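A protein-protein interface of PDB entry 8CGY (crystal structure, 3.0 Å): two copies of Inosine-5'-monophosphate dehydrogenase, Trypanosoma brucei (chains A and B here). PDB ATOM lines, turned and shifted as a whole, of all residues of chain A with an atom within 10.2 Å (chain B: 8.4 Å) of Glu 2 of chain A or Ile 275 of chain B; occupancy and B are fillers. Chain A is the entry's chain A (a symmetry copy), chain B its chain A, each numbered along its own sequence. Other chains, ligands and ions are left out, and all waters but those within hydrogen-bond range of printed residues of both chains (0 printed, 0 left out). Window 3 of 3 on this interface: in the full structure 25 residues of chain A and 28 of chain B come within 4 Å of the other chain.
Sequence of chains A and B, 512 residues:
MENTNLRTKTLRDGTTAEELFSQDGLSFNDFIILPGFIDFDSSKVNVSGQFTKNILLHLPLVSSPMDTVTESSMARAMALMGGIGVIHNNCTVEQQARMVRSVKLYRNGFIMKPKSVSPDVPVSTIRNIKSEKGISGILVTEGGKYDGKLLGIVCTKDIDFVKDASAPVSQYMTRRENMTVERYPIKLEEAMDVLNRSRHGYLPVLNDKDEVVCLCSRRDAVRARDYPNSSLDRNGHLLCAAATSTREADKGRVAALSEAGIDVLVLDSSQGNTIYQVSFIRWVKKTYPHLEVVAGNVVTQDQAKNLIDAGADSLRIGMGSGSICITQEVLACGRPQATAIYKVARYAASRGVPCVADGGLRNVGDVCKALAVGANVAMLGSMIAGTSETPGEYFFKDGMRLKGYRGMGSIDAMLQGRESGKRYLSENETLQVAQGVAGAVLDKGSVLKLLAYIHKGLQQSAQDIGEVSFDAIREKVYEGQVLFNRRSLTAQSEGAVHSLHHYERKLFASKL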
ATOM      1  N   GLU A   2      11.812  -6.379  -6.077  1.00  0.00           N
ATOM      2  CA  GLU A   2      11.285  -7.737  -6.030  1.00  0.00           C
ATOM      3  C   GLU A   2      12.072  -8.554  -5.023  1.00  0.00           C
ATOM      4  O   GLU A   2      12.459  -9.690  -5.291  1.00  0.00           O
ATOM      5  CB  GLU A   2      11.349  -8.394  -7.409  1.00  0.00           C
ATOM      6  N   ASN A   3      12.308  -7.974  -3.861  1.00  0.00           N
ATOM      7  CA  ASN A   3      13.215  -8.561  -2.893  1.00  0.00           C
ATOM      8  C   ASN A   3      12.462  -8.898  -1.609  1.00  0.00           C
ATOM      9  O   ASN A   3      11.228  -8.873  -1.552  1.00  0.00           O
ATOM     10  CB  ASN A   3      14.400  -7.629  -2.636  1.00  0.00           C
ATOM     11  CG  ASN A   3      15.348  -7.551  -3.819  1.00  0.00           C
ATOM     12  OD1 ASN A   3      15.508  -8.516  -4.568  1.00  0.00           O
ATOM     13  ND2 ASN A   3      15.985  -6.399  -3.992  1.00  0.00           N
ATOM     14  N   THR A   4      13.238  -9.240  -0.580  1.00  0.00           N
ATOM     15  CA  THR A   4      12.675  -9.724   0.673  1.00  0.00           C
ATOM     16  C   THR A   4      11.742  -8.713   1.323  1.00  0.00           C
ATOM     17  O   THR A   4      10.804  -9.103   2.026  1.00  0.00           O
ATOM     18  CB  THR A   4      13.799 -10.070   1.644  1.00  0.00           C
ATOM     19  OG1 THR A   4      14.537  -8.879   1.953  1.00  0.00           O
ATOM     20  CG2 THR A   4      14.737 -11.091   1.024  1.00  0.00           C
ATOM     21  N   ASN A   5      11.985  -7.417   1.133  1.00  0.00           N
ATOM     22  CA  ASN A   5      11.160  -6.442   1.840  1.00  0.00           C
ATOM     23  C   ASN A   5       9.705  -6.528   1.396  1.00  0.00           C
ATOM     24  O   ASN A   5       8.792  -6.419   2.224  1.00  0.00           O
ATOM     25  CB  ASN A   5      11.698  -5.027   1.648  1.00  0.00           C
ATOM     26  CG  ASN A   5      11.022  -4.030   2.565  1.00  0.00           C
ATOM     27  OD1 ASN A   5      11.436  -3.839   3.709  1.00  0.00           O
ATOM     28  ND2 ASN A   5       9.953  -3.413   2.078  1.00  0.00           N
ATOM     29  N   LEU A   6       9.467  -6.737   0.098  1.00  0.00           N
ATOM     30  CA  LEU A   6       8.105  -6.848  -0.410  1.00  0.00           C
ATOM     31  C   LEU A   6       7.471  -8.211  -0.148  1.00  0.00           C
ATOM     32  O   LEU A   6       6.244  -8.329  -0.241  1.00  0.00           O
ATOM     33  CB  LEU A   6       8.078  -6.561  -1.916  1.00  0.00           C
ATOM     34  CG  LEU A   6       8.381  -5.148  -2.430  1.00  0.00           C
ATOM     35  CD1 LEU A   6       9.106  -5.207  -3.765  1.00  0.00           C
ATOM     36  CD2 LEU A   6       7.099  -4.353  -2.578  1.00  0.00           C
ATOM     37  N   ARG A   7       8.259  -9.238   0.177  1.00  0.00           N
ATOM     38  CA  ARG A   7       7.699 -10.576   0.369  1.00  0.00           C
ATOM     39  C   ARG A   7       7.421 -10.927   1.824  1.00  0.00           C
ATOM     40  O   ARG A   7       6.459 -11.648   2.100  1.00  0.00           O
ATOM     41  CB  ARG A   7       8.625 -11.650  -0.218  1.00  0.00           C
ATOM     42  CG  ARG A   7       8.052 -13.071  -0.095  1.00  0.00           C
ATOM     43  CD  ARG A   7       8.995 -14.127  -0.661  1.00  0.00           C
ATOM     44  NE  ARG A   7       9.625 -13.670  -1.893  1.00  0.00           N
ATOM     45  CZ  ARG A   7       9.051 -13.694  -3.087  1.00  0.00           C
ATOM     46  NH1 ARG A   7       7.834 -14.182  -3.259  1.00  0.00           N
ATOM     47  NH2 ARG A   7       9.711 -13.207  -4.133  1.00  0.00           N
ATOM     48  N   THR A   8       8.242 -10.467   2.765  1.00  0.00           N
ATOM     49  CA  THR A   8       8.060 -10.900   4.141  1.00  0.00           C
ATOM     50  C   THR A   8       6.837 -10.224   4.744  1.00  0.00           C
ATOM     51  O   THR A   8       6.705  -8.996   4.710  1.00  0.00           O
ATOM     52  CB  THR A   8       9.300 -10.597   4.987  1.00  0.00           C
ATOM     53  OG1 THR A   8       9.584  -9.193   4.952  1.00  0.00           O
ATOM     54  CG2 THR A   8      10.503 -11.375   4.465  1.00  0.00           C
ATOM     55  N   GLY A  36       0.328 -14.689  -1.565  1.00  0.00           N
ATOM     56  CA  GLY A  36       1.552 -14.025  -1.149  1.00  0.00           C
ATOM     57  C   GLY A  36       2.024 -12.942  -2.102  1.00  0.00           C
ATOM     58  O   GLY A  36       1.247 -12.049  -2.450  1.00  0.00           O
ATOM     59  N   PHE A  37       3.290 -12.995  -2.526  1.00  0.00           N
ATOM     60  CA  PHE A  37       3.871 -11.975  -3.395  1.00  0.00           C
ATOM     61  C   PHE A  37       4.595 -12.627  -4.566  1.00  0.00           C
ATOM     62  O   PHE A  37       5.439 -13.508  -4.368  1.00  0.00           O
ATOM     63  CB  PHE A  37       4.840 -11.073  -2.621  1.00  0.00           C
ATOM     64  CG  PHE A  37       5.562 -10.074  -3.488  1.00  0.00           C
ATOM     65  CD1 PHE A  37       5.007  -8.833  -3.747  1.00  0.00           C
ATOM     66  CD2 PHE A  37       6.798 -10.379  -4.041  1.00  0.00           C
ATOM     67  CE1 PHE A  37       5.670  -7.912  -4.544  1.00  0.00           C
ATOM     68  CE2 PHE A  37       7.465  -9.465  -4.839  1.00  0.00           C
ATOM     69  CZ  PHE A  37       6.900  -8.230  -5.089  1.00  0.00           C
ATOM     70  N   ILE A  38       4.297 -12.154  -5.776  1.00  0.00           N
ATOM     71  CA  ILE A  38       4.734 -12.780  -7.022  1.00  0.00           C
ATOM     72  C   ILE A  38       5.799 -11.909  -7.673  1.00  0.00           C
ATOM     73  O   ILE A  38       5.602 -10.699  -7.841  1.00  0.00           O
ATOM     74  CB  ILE A  38       3.542 -12.986  -7.971  1.00  0.00           C
ATOM     75  CG1 ILE A  38       2.445 -13.783  -7.264  1.00  0.00           C
ATOM     76  CG2 ILE A  38       3.980 -13.670  -9.258  1.00  0.00           C
ATOM     77  CD1 ILE A  38       1.326 -14.215  -8.169  1.00  0.00           C
ATOM     78  N   ASP A  39       6.947 -12.511  -7.993  1.00  0.00           N
ATOM     79  CA  ASP A  39       7.976 -11.877  -8.820  1.00  0.00           C
ATOM     80  C   ASP A  39       8.623 -12.894  -9.758  1.00  0.00           C
ATOM     81  O   ASP A  39       9.850 -12.938  -9.900  1.00  0.00           O
ATOM     82  CB  ASP A  39       9.027 -11.168  -7.961  1.00  0.00           C
ATOM     83  CG  ASP A  39       9.688 -12.087  -6.949  1.00  0.00           C
ATOM     84  OD1 ASP A  39       9.401 -13.299  -6.959  1.00  0.00           O
ATOM     85  OD2 ASP A  39      10.497 -11.590  -6.139  1.00  0.00           O
ATOM     86  N   PHE A  40       7.814 -13.729 -10.404  1.00  0.00           N
ATOM     87  CA  PHE A  40       8.378 -14.798 -11.218  1.00  0.00           C
ATOM     88  C   PHE A  40       7.267 -15.482 -11.998  1.00  0.00           C
ATOM     89  O   PHE A  40       6.113 -15.502 -11.559  1.00  0.00           O
ATOM     90  CB  PHE A  40       9.117 -15.811 -10.337  1.00  0.00           C
ATOM     91  CG  PHE A  40       8.279 -16.362  -9.214  1.00  0.00           C
ATOM     92  CD1 PHE A  40       8.238 -15.731  -7.979  1.00  0.00           C
ATOM     93  CD2 PHE A  40       7.528 -17.513  -9.395  1.00  0.00           C
ATOM     94  CE1 PHE A  40       7.468 -16.240  -6.942  1.00  0.00           C
ATOM     95  CE2 PHE A  40       6.757 -18.028  -8.365  1.00  0.00           C
ATOM     96  CZ  PHE A  40       6.728 -17.390  -7.137  1.00  0.00           C
ATOM     97  N   ASP A  41       7.619 -16.032 -13.157  1.00  0.00           N
ATOM     98  CA  ASP A  41       6.656 -16.802 -13.930  1.00  0.00           C
ATOM     99  C   ASP A  41       6.495 -18.191 -13.319  1.00  0.00           C
ATOM    100  O   ASP A  41       7.431 -18.747 -12.740  1.00  0.00           O
ATOM    101  CB  ASP A  41       7.091 -16.906 -15.393  1.00  0.00           C
ATOM    102  CG  ASP A  41       7.298 -15.543 -16.044  1.00  0.00           C
ATOM    103  OD1 ASP A  41       6.481 -14.628 -15.800  1.00  0.00           O
ATOM    104  OD2 ASP A  41       8.283 -15.385 -16.796  1.00  0.00           O
ATOM    105  N   GLN A 463       2.700 -20.188  -7.537  1.00  0.00           N
ATOM    106  CA  GLN A 463       2.880 -18.785  -7.898  1.00  0.00           C
ATOM    107  C   GLN A 463       1.941 -17.892  -7.096  1.00  0.00           C
ATOM    108  O   GLN A 463       2.363 -16.871  -6.540  1.00  0.00           O
ATOM    109  CB  GLN A 463       2.665 -18.582  -9.396  1.00  0.00           C
ATOM    110  CG  GLN A 463       2.949 -17.157  -9.847  1.00  0.00           C
ATOM    111  CD  GLN A 463       2.558 -16.913 -11.286  1.00  0.00           C
ATOM    112  OE1 GLN A 463       1.442 -17.228 -11.696  1.00  0.00           O
ATOM    113  NE2 GLN A 463       3.478 -16.355 -12.062  1.00  0.00           N
ATOM    114  N   GLY A 466       3.009 -17.472  -3.601  1.00  0.00           N
ATOM    115  CA  GLY A 466       4.117 -16.535  -3.542  1.00  0.00           C
ATOM    116  C   GLY A 466       5.494 -17.110  -3.278  1.00  0.00           C
ATOM    117  O   GLY A 466       6.388 -16.353  -2.880  1.00  0.00           O
ATOM    118  N   VAL A 468       8.630 -19.878  -4.893  1.00  0.00           N
ATOM    119  CA  VAL A 468       9.061 -20.479  -6.156  1.00  0.00           C
ATOM    120  C   VAL A 468       9.415 -21.945  -5.970  1.00  0.00           C
ATOM    121  O   VAL A 468      10.000 -22.572  -6.861  1.00  0.00           O
ATOM    122  CB  VAL A 468      10.271 -19.750  -6.769  1.00  0.00           C
ATOM    123  CG1 VAL A 468       9.981 -18.277  -6.974  1.00  0.00           C
ATOM    124  CG2 VAL A 468      11.518 -19.976  -5.916  1.00  0.00           C
ATOM    125  N   THR B 246      -1.247  -5.118 -16.201  1.00  0.00           N
ATOM    126  CA  THR B 246      -0.053  -4.415 -15.751  1.00  0.00           C
ATOM    127  C   THR B 246       1.192  -4.802 -16.533  1.00  0.00           C
ATOM    128  O   THR B 246       2.303  -4.477 -16.104  1.00  0.00           O
ATOM    129  CB  THR B 246       0.183  -4.678 -14.265  1.00  0.00           C
ATOM    130  OG1 THR B 246       0.407  -6.080 -14.066  1.00  0.00           O
ATOM    131  CG2 THR B 246      -1.020  -4.234 -13.453  1.00  0.00           C
ATOM    132  N   GLN B 271      -4.561 -11.976  -8.651  1.00  0.00           N
ATOM    133  CA  GLN B 271      -3.816 -11.483  -7.500  1.00  0.00           C
ATOM    134  C   GLN B 271      -2.916 -10.345  -7.940  1.00  0.00           C
ATOM    135  O   GLN B 271      -2.062 -10.530  -8.814  1.00  0.00           O
ATOM    136  CB  GLN B 271      -2.954 -12.550  -6.853  1.00  0.00           C
ATOM    137  CG  GLN B 271      -1.889 -11.866  -6.034  1.00  0.00           C
ATOM    138  CD  GLN B 271      -1.123 -12.827  -5.208  1.00  0.00           C
ATOM    139  OE1 GLN B 271      -1.507 -13.987  -5.095  1.00  0.00           O
ATOM    140  NE2 GLN B 271      -0.026 -12.371  -4.623  1.00  0.00           N
ATOM    141  N   GLY B 272      -3.067  -9.197  -7.297  1.00  0.00           N
ATOM    142  CA  GLY B 272      -2.372  -8.004  -7.714  1.00  0.00           C
ATOM    143  C   GLY B 272      -1.117  -7.684  -6.948  1.00  0.00           C
ATOM    144  O   GLY B 272      -0.508  -6.642  -7.201  1.00  0.00           O
ATOM    145  N   ASN B 273      -0.705  -8.542  -6.017  1.00  0.00           N
ATOM    146  CA  ASN B 273       0.478  -8.287  -5.202  1.00  0.00           C
ATOM    147  C   ASN B 273       1.679  -8.844  -5.959  1.00  0.00           C
ATOM    148  O   ASN B 273       2.224  -9.909  -5.642  1.00  0.00           O
ATOM    149  CB  ASN B 273       0.305  -8.908  -3.821  1.00  0.00           C
ATOM    150  CG  ASN B 273       1.400  -8.508  -2.860  1.00  0.00           C
ATOM    151  OD1 ASN B 273       2.029  -7.460  -3.010  1.00  0.00           O
ATOM    152  ND2 ASN B 273       1.631  -9.346  -1.859  1.00  0.00           N
ATOM    153  N   THR B 274       2.101  -8.116  -6.991  1.00  0.00           N
ATOM    154  CA  THR B 274       3.167  -8.567  -7.867  1.00  0.00           C
ATOM    155  C   THR B 274       4.140  -7.427  -8.119  1.00  0.00           C
ATOM    156  O   THR B 274       3.779  -6.248  -8.044  1.00  0.00           O
ATOM    157  CB  THR B 274       2.622  -9.109  -9.213  1.00  0.00           C
ATOM    158  OG1 THR B 274       2.342  -8.026 -10.109  1.00  0.00           O
ATOM    159  CG2 THR B 274       1.355  -9.925  -8.989  1.00  0.00           C
ATOM    160  N   ILE B 275       5.391  -7.793  -8.400  1.00  0.00           N
ATOM    161  CA  ILE B 275       6.379  -6.768  -8.706  1.00  0.00           C
ATOM    162  C   ILE B 275       5.929  -5.982  -9.924  1.00  0.00           C
ATOM    163  O   ILE B 275       6.191  -4.777 -10.038  1.00  0.00           O
ATOM    164  CB  ILE B 275       7.769  -7.408  -8.900  1.00  0.00           C
ATOM    165  CG1 ILE B 275       8.829  -6.336  -9.149  1.00  0.00           C
ATOM    166  CG2 ILE B 275       7.742  -8.443 -10.019  1.00  0.00           C
ATOM    167  CD1 ILE B 275       8.923  -5.321  -8.033  1.00  0.00           C
ATOM    168  N   TYR B 276       5.201  -6.639 -10.823  1.00  0.00           N
ATOM    169  CA  TYR B 276       4.751  -6.002 -12.053  1.00  0.00           C
ATOM    170  C   TYR B 276       3.681  -4.957 -11.776  1.00  0.00           C
ATOM    171  O   TYR B 276       3.729  -3.844 -12.312  1.00  0.00           O
ATOM    172  CB  TYR B 276       4.239  -7.079 -13.006  1.00  0.00           C
ATOM    173  CG  TYR B 276       5.123  -8.308 -12.977  1.00  0.00           C
ATOM    174  CD1 TYR B 276       6.403  -8.272 -13.513  1.00  0.00           C
ATOM    175  CD2 TYR B 276       4.694  -9.493 -12.389  1.00  0.00           C
ATOM    176  CE1 TYR B 276       7.228  -9.383 -13.481  1.00  0.00           C
ATOM    177  CE2 TYR B 276       5.512 -10.613 -12.354  1.00  0.00           C
ATOM    178  CZ  TYR B 276       6.779 -10.551 -12.903  1.00  0.00           C
ATOM    179  OH  TYR B 276       7.600 -11.656 -12.872  1.00  0.00           O
ATOM    180  N   GLN B 277       2.706  -5.292 -10.934  1.00  0.00           N
ATOM    181  CA  GLN B 277       1.671  -4.322 -10.616  1.00  0.00           C
ATOM    182  C   GLN B 277       2.241  -3.152  -9.832  1.00  0.00           C
ATOM    183  O   GLN B 277       1.831  -2.004 -10.027  1.00  0.00           O
ATOM    184  CB  GLN B 277       0.544  -4.984  -9.834  1.00  0.00           C
ATOM    185  CG  GLN B 277      -0.505  -3.989  -9.433  1.00  0.00           C
ATOM    186  CD  GLN B 277      -1.876  -4.599  -9.341  1.00  0.00           C
ATOM    187  OE1 GLN B 277      -2.687  -4.190  -8.517  1.00  0.00           O
ATOM    188  NE2 GLN B 277      -2.152  -5.579 -10.196  1.00  0.00           N
ATOM    189  N   VAL B 278       3.196  -3.428  -8.945  1.00  0.00           N
ATOM    190  CA  VAL B 278       3.831  -2.364  -8.172  1.00  0.00           C
ATOM    191  C   VAL B 278       4.533  -1.375  -9.098  1.00  0.00           C
ATOM    192  O   VAL B 278       4.340  -0.158  -8.988  1.00  0.00           O
ATOM    193  CB  VAL B 278       4.794  -2.968  -7.134  1.00  0.00           C
ATOM    194  CG1 VAL B 278       5.668  -1.891  -6.521  1.00  0.00           C
ATOM    195  CG2 VAL B 278       4.000  -3.699  -6.058  1.00  0.00           C
ATOM    196  N   SER B 279       5.342  -1.874 -10.040  1.00  0.00           N
ATOM    197  CA  SER B 279       5.996  -0.963 -10.978  1.00  0.00           C
ATOM    198  C   SER B 279       4.962  -0.160 -11.750  1.00  0.00           C
ATOM    199  O   SER B 279       5.089   1.060 -11.904  1.00  0.00           O
ATOM    200  CB  SER B 279       6.885  -1.724 -11.962  1.00  0.00           C
ATOM    201  OG  SER B 279       7.701  -2.675 -11.317  1.00  0.00           O
ATOM    202  N   PHE B 280       3.927  -0.841 -12.239  1.00  0.00           N
ATOM    203  CA  PHE B 280       2.922  -0.197 -13.072  1.00  0.00           C
ATOM    204  C   PHE B 280       2.296   0.984 -12.346  1.00  0.00           C
ATOM    205  O   PHE B 280       2.209   2.090 -12.892  1.00  0.00           O
ATOM    206  CB  PHE B 280       1.864  -1.229 -13.472  1.00  0.00           C
ATOM    207  CG  PHE B 280       1.194  -0.947 -14.783  1.00  0.00           C
ATOM    208  CD1 PHE B 280       1.859  -1.168 -15.979  1.00  0.00           C
ATOM    209  CD2 PHE B 280      -0.105  -0.474 -14.820  1.00  0.00           C
ATOM    210  CE1 PHE B 280       1.242  -0.910 -17.189  1.00  0.00           C
ATOM    211  CE2 PHE B 280      -0.727  -0.215 -16.026  1.00  0.00           C
ATOM    212  CZ  PHE B 280      -0.052  -0.433 -17.212  1.00  0.00           C
ATOM    213  N   ILE B 281       1.892   0.776 -11.091  1.00  0.00           N
ATOM    214  CA  ILE B 281       1.280   1.850 -10.314  1.00  0.00           C
ATOM    215  C   ILE B 281       2.226   3.036 -10.212  1.00  0.00           C
ATOM    216  O   ILE B 281       1.826   4.192 -10.396  1.00  0.00           O
ATOM    217  CB  ILE B 281       0.885   1.344  -8.917  1.00  0.00           C
ATOM    218  CG1 ILE B 281      -0.184   0.261  -9.020  1.00  0.00           C
ATOM    219  CG2 ILE B 281       0.416   2.505  -8.056  1.00  0.00           C
ATOM    220  CD1 ILE B 281      -0.581  -0.309  -7.682  1.00  0.00           C
ATOM    221  N   ARG B 282       3.494   2.772  -9.892  1.00  0.00           N
ATOM    222  CA  ARG B 282       4.450   3.868  -9.780  1.00  0.00           C
ATOM    223  C   ARG B 282       4.602   4.586 -11.110  1.00  0.00           C
ATOM    224  O   ARG B 282       4.677   5.819 -11.156  1.00  0.00           O
ATOM    225  CB  ARG B 282       5.799   3.349  -9.279  1.00  0.00           C
ATOM    226  CG  ARG B 282       5.902   3.313  -7.763  1.00  0.00           C
ATOM    227  CD  ARG B 282       7.152   2.599  -7.272  1.00  0.00           C
ATOM    228  NE  ARG B 282       6.957   2.121  -5.908  1.00  0.00           N
ATOM    229  CZ  ARG B 282       7.560   1.064  -5.384  1.00  0.00           C
ATOM    230  NH1 ARG B 282       8.458   0.372  -6.062  1.00  0.00           N
ATOM    231  NH2 ARG B 282       7.239   0.680  -4.156  1.00  0.00           N
ATOM    232  N   ASN B 306       1.413  -3.468   0.282  1.00  0.00           N
ATOM    233  CA  ASN B 306       2.339  -3.271  -0.827  1.00  0.00           C
ATOM    234  C   ASN B 306       1.745  -2.356  -1.892  1.00  0.00           C
ATOM    235  O   ASN B 306       2.406  -1.429  -2.374  1.00  0.00           O
ATOM    236  CB  ASN B 306       2.736  -4.622  -1.415  1.00  0.00           C
ATOM    237  CG  ASN B 306       3.980  -5.182  -0.763  1.00  0.00           C
ATOM    238  OD1 ASN B 306       4.726  -4.455  -0.105  1.00  0.00           O
ATOM    239  ND2 ASN B 306       4.220  -6.473  -0.949  1.00  0.00           N
ATOM    240  N   LEU B 307       0.484  -2.590  -2.265  1.00  0.00           N
ATOM    241  CA  LEU B 307      -0.132  -1.786  -3.317  1.00  0.00           C
ATOM    242  C   LEU B 307      -0.406  -0.358  -2.861  1.00  0.00           C
ATOM    243  O   LEU B 307      -0.301   0.575  -3.667  1.00  0.00           O
ATOM    244  CB  LEU B 307      -1.417  -2.463  -3.800  1.00  0.00           C
ATOM    245  CG  LEU B 307      -1.229  -3.851  -4.428  1.00  0.00           C
ATOM    246  CD1 LEU B 307      -2.522  -4.352  -5.058  1.00  0.00           C
ATOM    247  CD2 LEU B 307      -0.097  -3.832  -5.450  1.00  0.00           C
ATOM    248  N   ALA B 310       2.809   1.748  -3.197  1.00  0.00           N
ATOM    249  CA  ALA B 310       3.120   2.162  -4.563  1.00  0.00           C
ATOM    250  C   ALA B 310       2.361   3.414  -4.990  1.00  0.00           C
ATOM    251  O   ALA B 310       2.770   4.068  -5.955  1.00  0.00           O
ATOM    252  CB  ALA B 310       2.820   1.024  -5.539  1.00  0.00           C
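Glu 2 of chain A touches one residue of chain B. Ile 275 of chain B touches four residues of chain A. Tyr 276 of chain B touches just these residues of chain A: Asp 39 and Phe 40. No residue of chain A comes within 4 Å of Val 278 of chain B. Printed residues of chain B within 4 Å of Gly 36 of chain A: Gln 271 and Asn 273. Of the printed residues of chain A, Gln 271 of chain B touches Gly 36, Phe 37 and Ile 38. Of the printed residues of chain B, Phe 40 of chain A touches Tyr 276. Printed residues of chain B within 4 Å of Phe 37 of chain A: Gln 271, Asn 273, Thr 274, Ile 275 and Asn 306. Arg 282 of chain B touches none of the printed residues of chain A. Phe 280 of chain B touches none of the printed residues of chain A.
No position is printed for both chains. Of the 16 pairs that touch across the chains among the printed residues, none has its exchanged pair printed and touching as well.
Of the 16 printed residues of chain A, 7 touch a printed residue of chain B. Hydrophobic or aromatic side chains of chain A that line the printed part of chain B: Leu 6, Phe 37 and Ile 38. Among the printed residues, no Asp or Glu carboxylate lies within 4 Å of a Lys or Arg side-chain nitrogen of the other chain.
NE2 of Gln 271 of chain B is in hydrogen-bond range of O of Gly 36 of chain A. ND2 of Asn 273 of chain B sits at hydrogen-bond distance from O of Gly 36 of chain A (2.8 Å). The backbone NH (N) of Ile 38 of chain A lies within hydrogen-bond range of the backbone carbonyl oxygen (O) of Asn 273 of chain B (3.1 Å). The backbone NH of Ile 275 of chain B sits at hydrogen-bond distance from the backbone carbonyl oxygen of Ile 38 of chain A (3.0 Å). The side-chain hydroxyl (OH) of Tyr 276 of chain B is in hydrogen-bond range of the backbone NH (N) of Phe 40 of chain A, 3.2 Å away. The side-chain amide nitrogen of Asn 306 of chain B lies within hydrogen-bond range of the backbone carbonyl oxygen of Leu 6 of chain A (2.8 Å).
The backbone carbonyl oxygen (O) of Asn 273 of chain B is in hydrogen-bond range of the side-chain amide nitrogen (NE2) of Gln 271 of chain B, at 3.5 Å. N of Tyr 276 of chain B sits close to OG1 of Thr 274 of chain B. The side-chain hydroxyl (OG1) of Thr 274 of chain B lies within hydrogen-bond range of the backbone NH (N) of Gln 277 of chain B. The backbone carbonyl oxygen of Ile 275 of chain B is in hydrogen-bond range of the side-chain hydroxyl of Ser 279 of chain B (2.9 Å). The guanidinium group of Arg 7 of chain A lies within hydrogen-bond range of the backbone carbonyl oxygen of Phe 37 of chain A, 2.7 Å away. NE2 of Gln 463 of chain A is in hydrogen-bond range of O of Phe 40 of chain A (2.8 Å).
Among the printed residues, pairs that only touch across the chains: Glu 2 of chain A with Ile 275 of chain B, Phe 37 of chain A with Gln 271 of chain B, Phe 37 of chain A with Asn 273 of chain B, Phe 37 of chain A with Thr 274 of chain B, Phe 37 of chain A with Ile 275 of chain B, Phe 37 of chain A with Asn 306 of chain B, Ile 38 of chain A with Gln 271 of chain B, Ile 38 of chain A with Thr 274 of chain B, Asp 39 of chain A with Ile 275 of chain B and Asp 39 of chain A with Tyr 276 of chain B.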
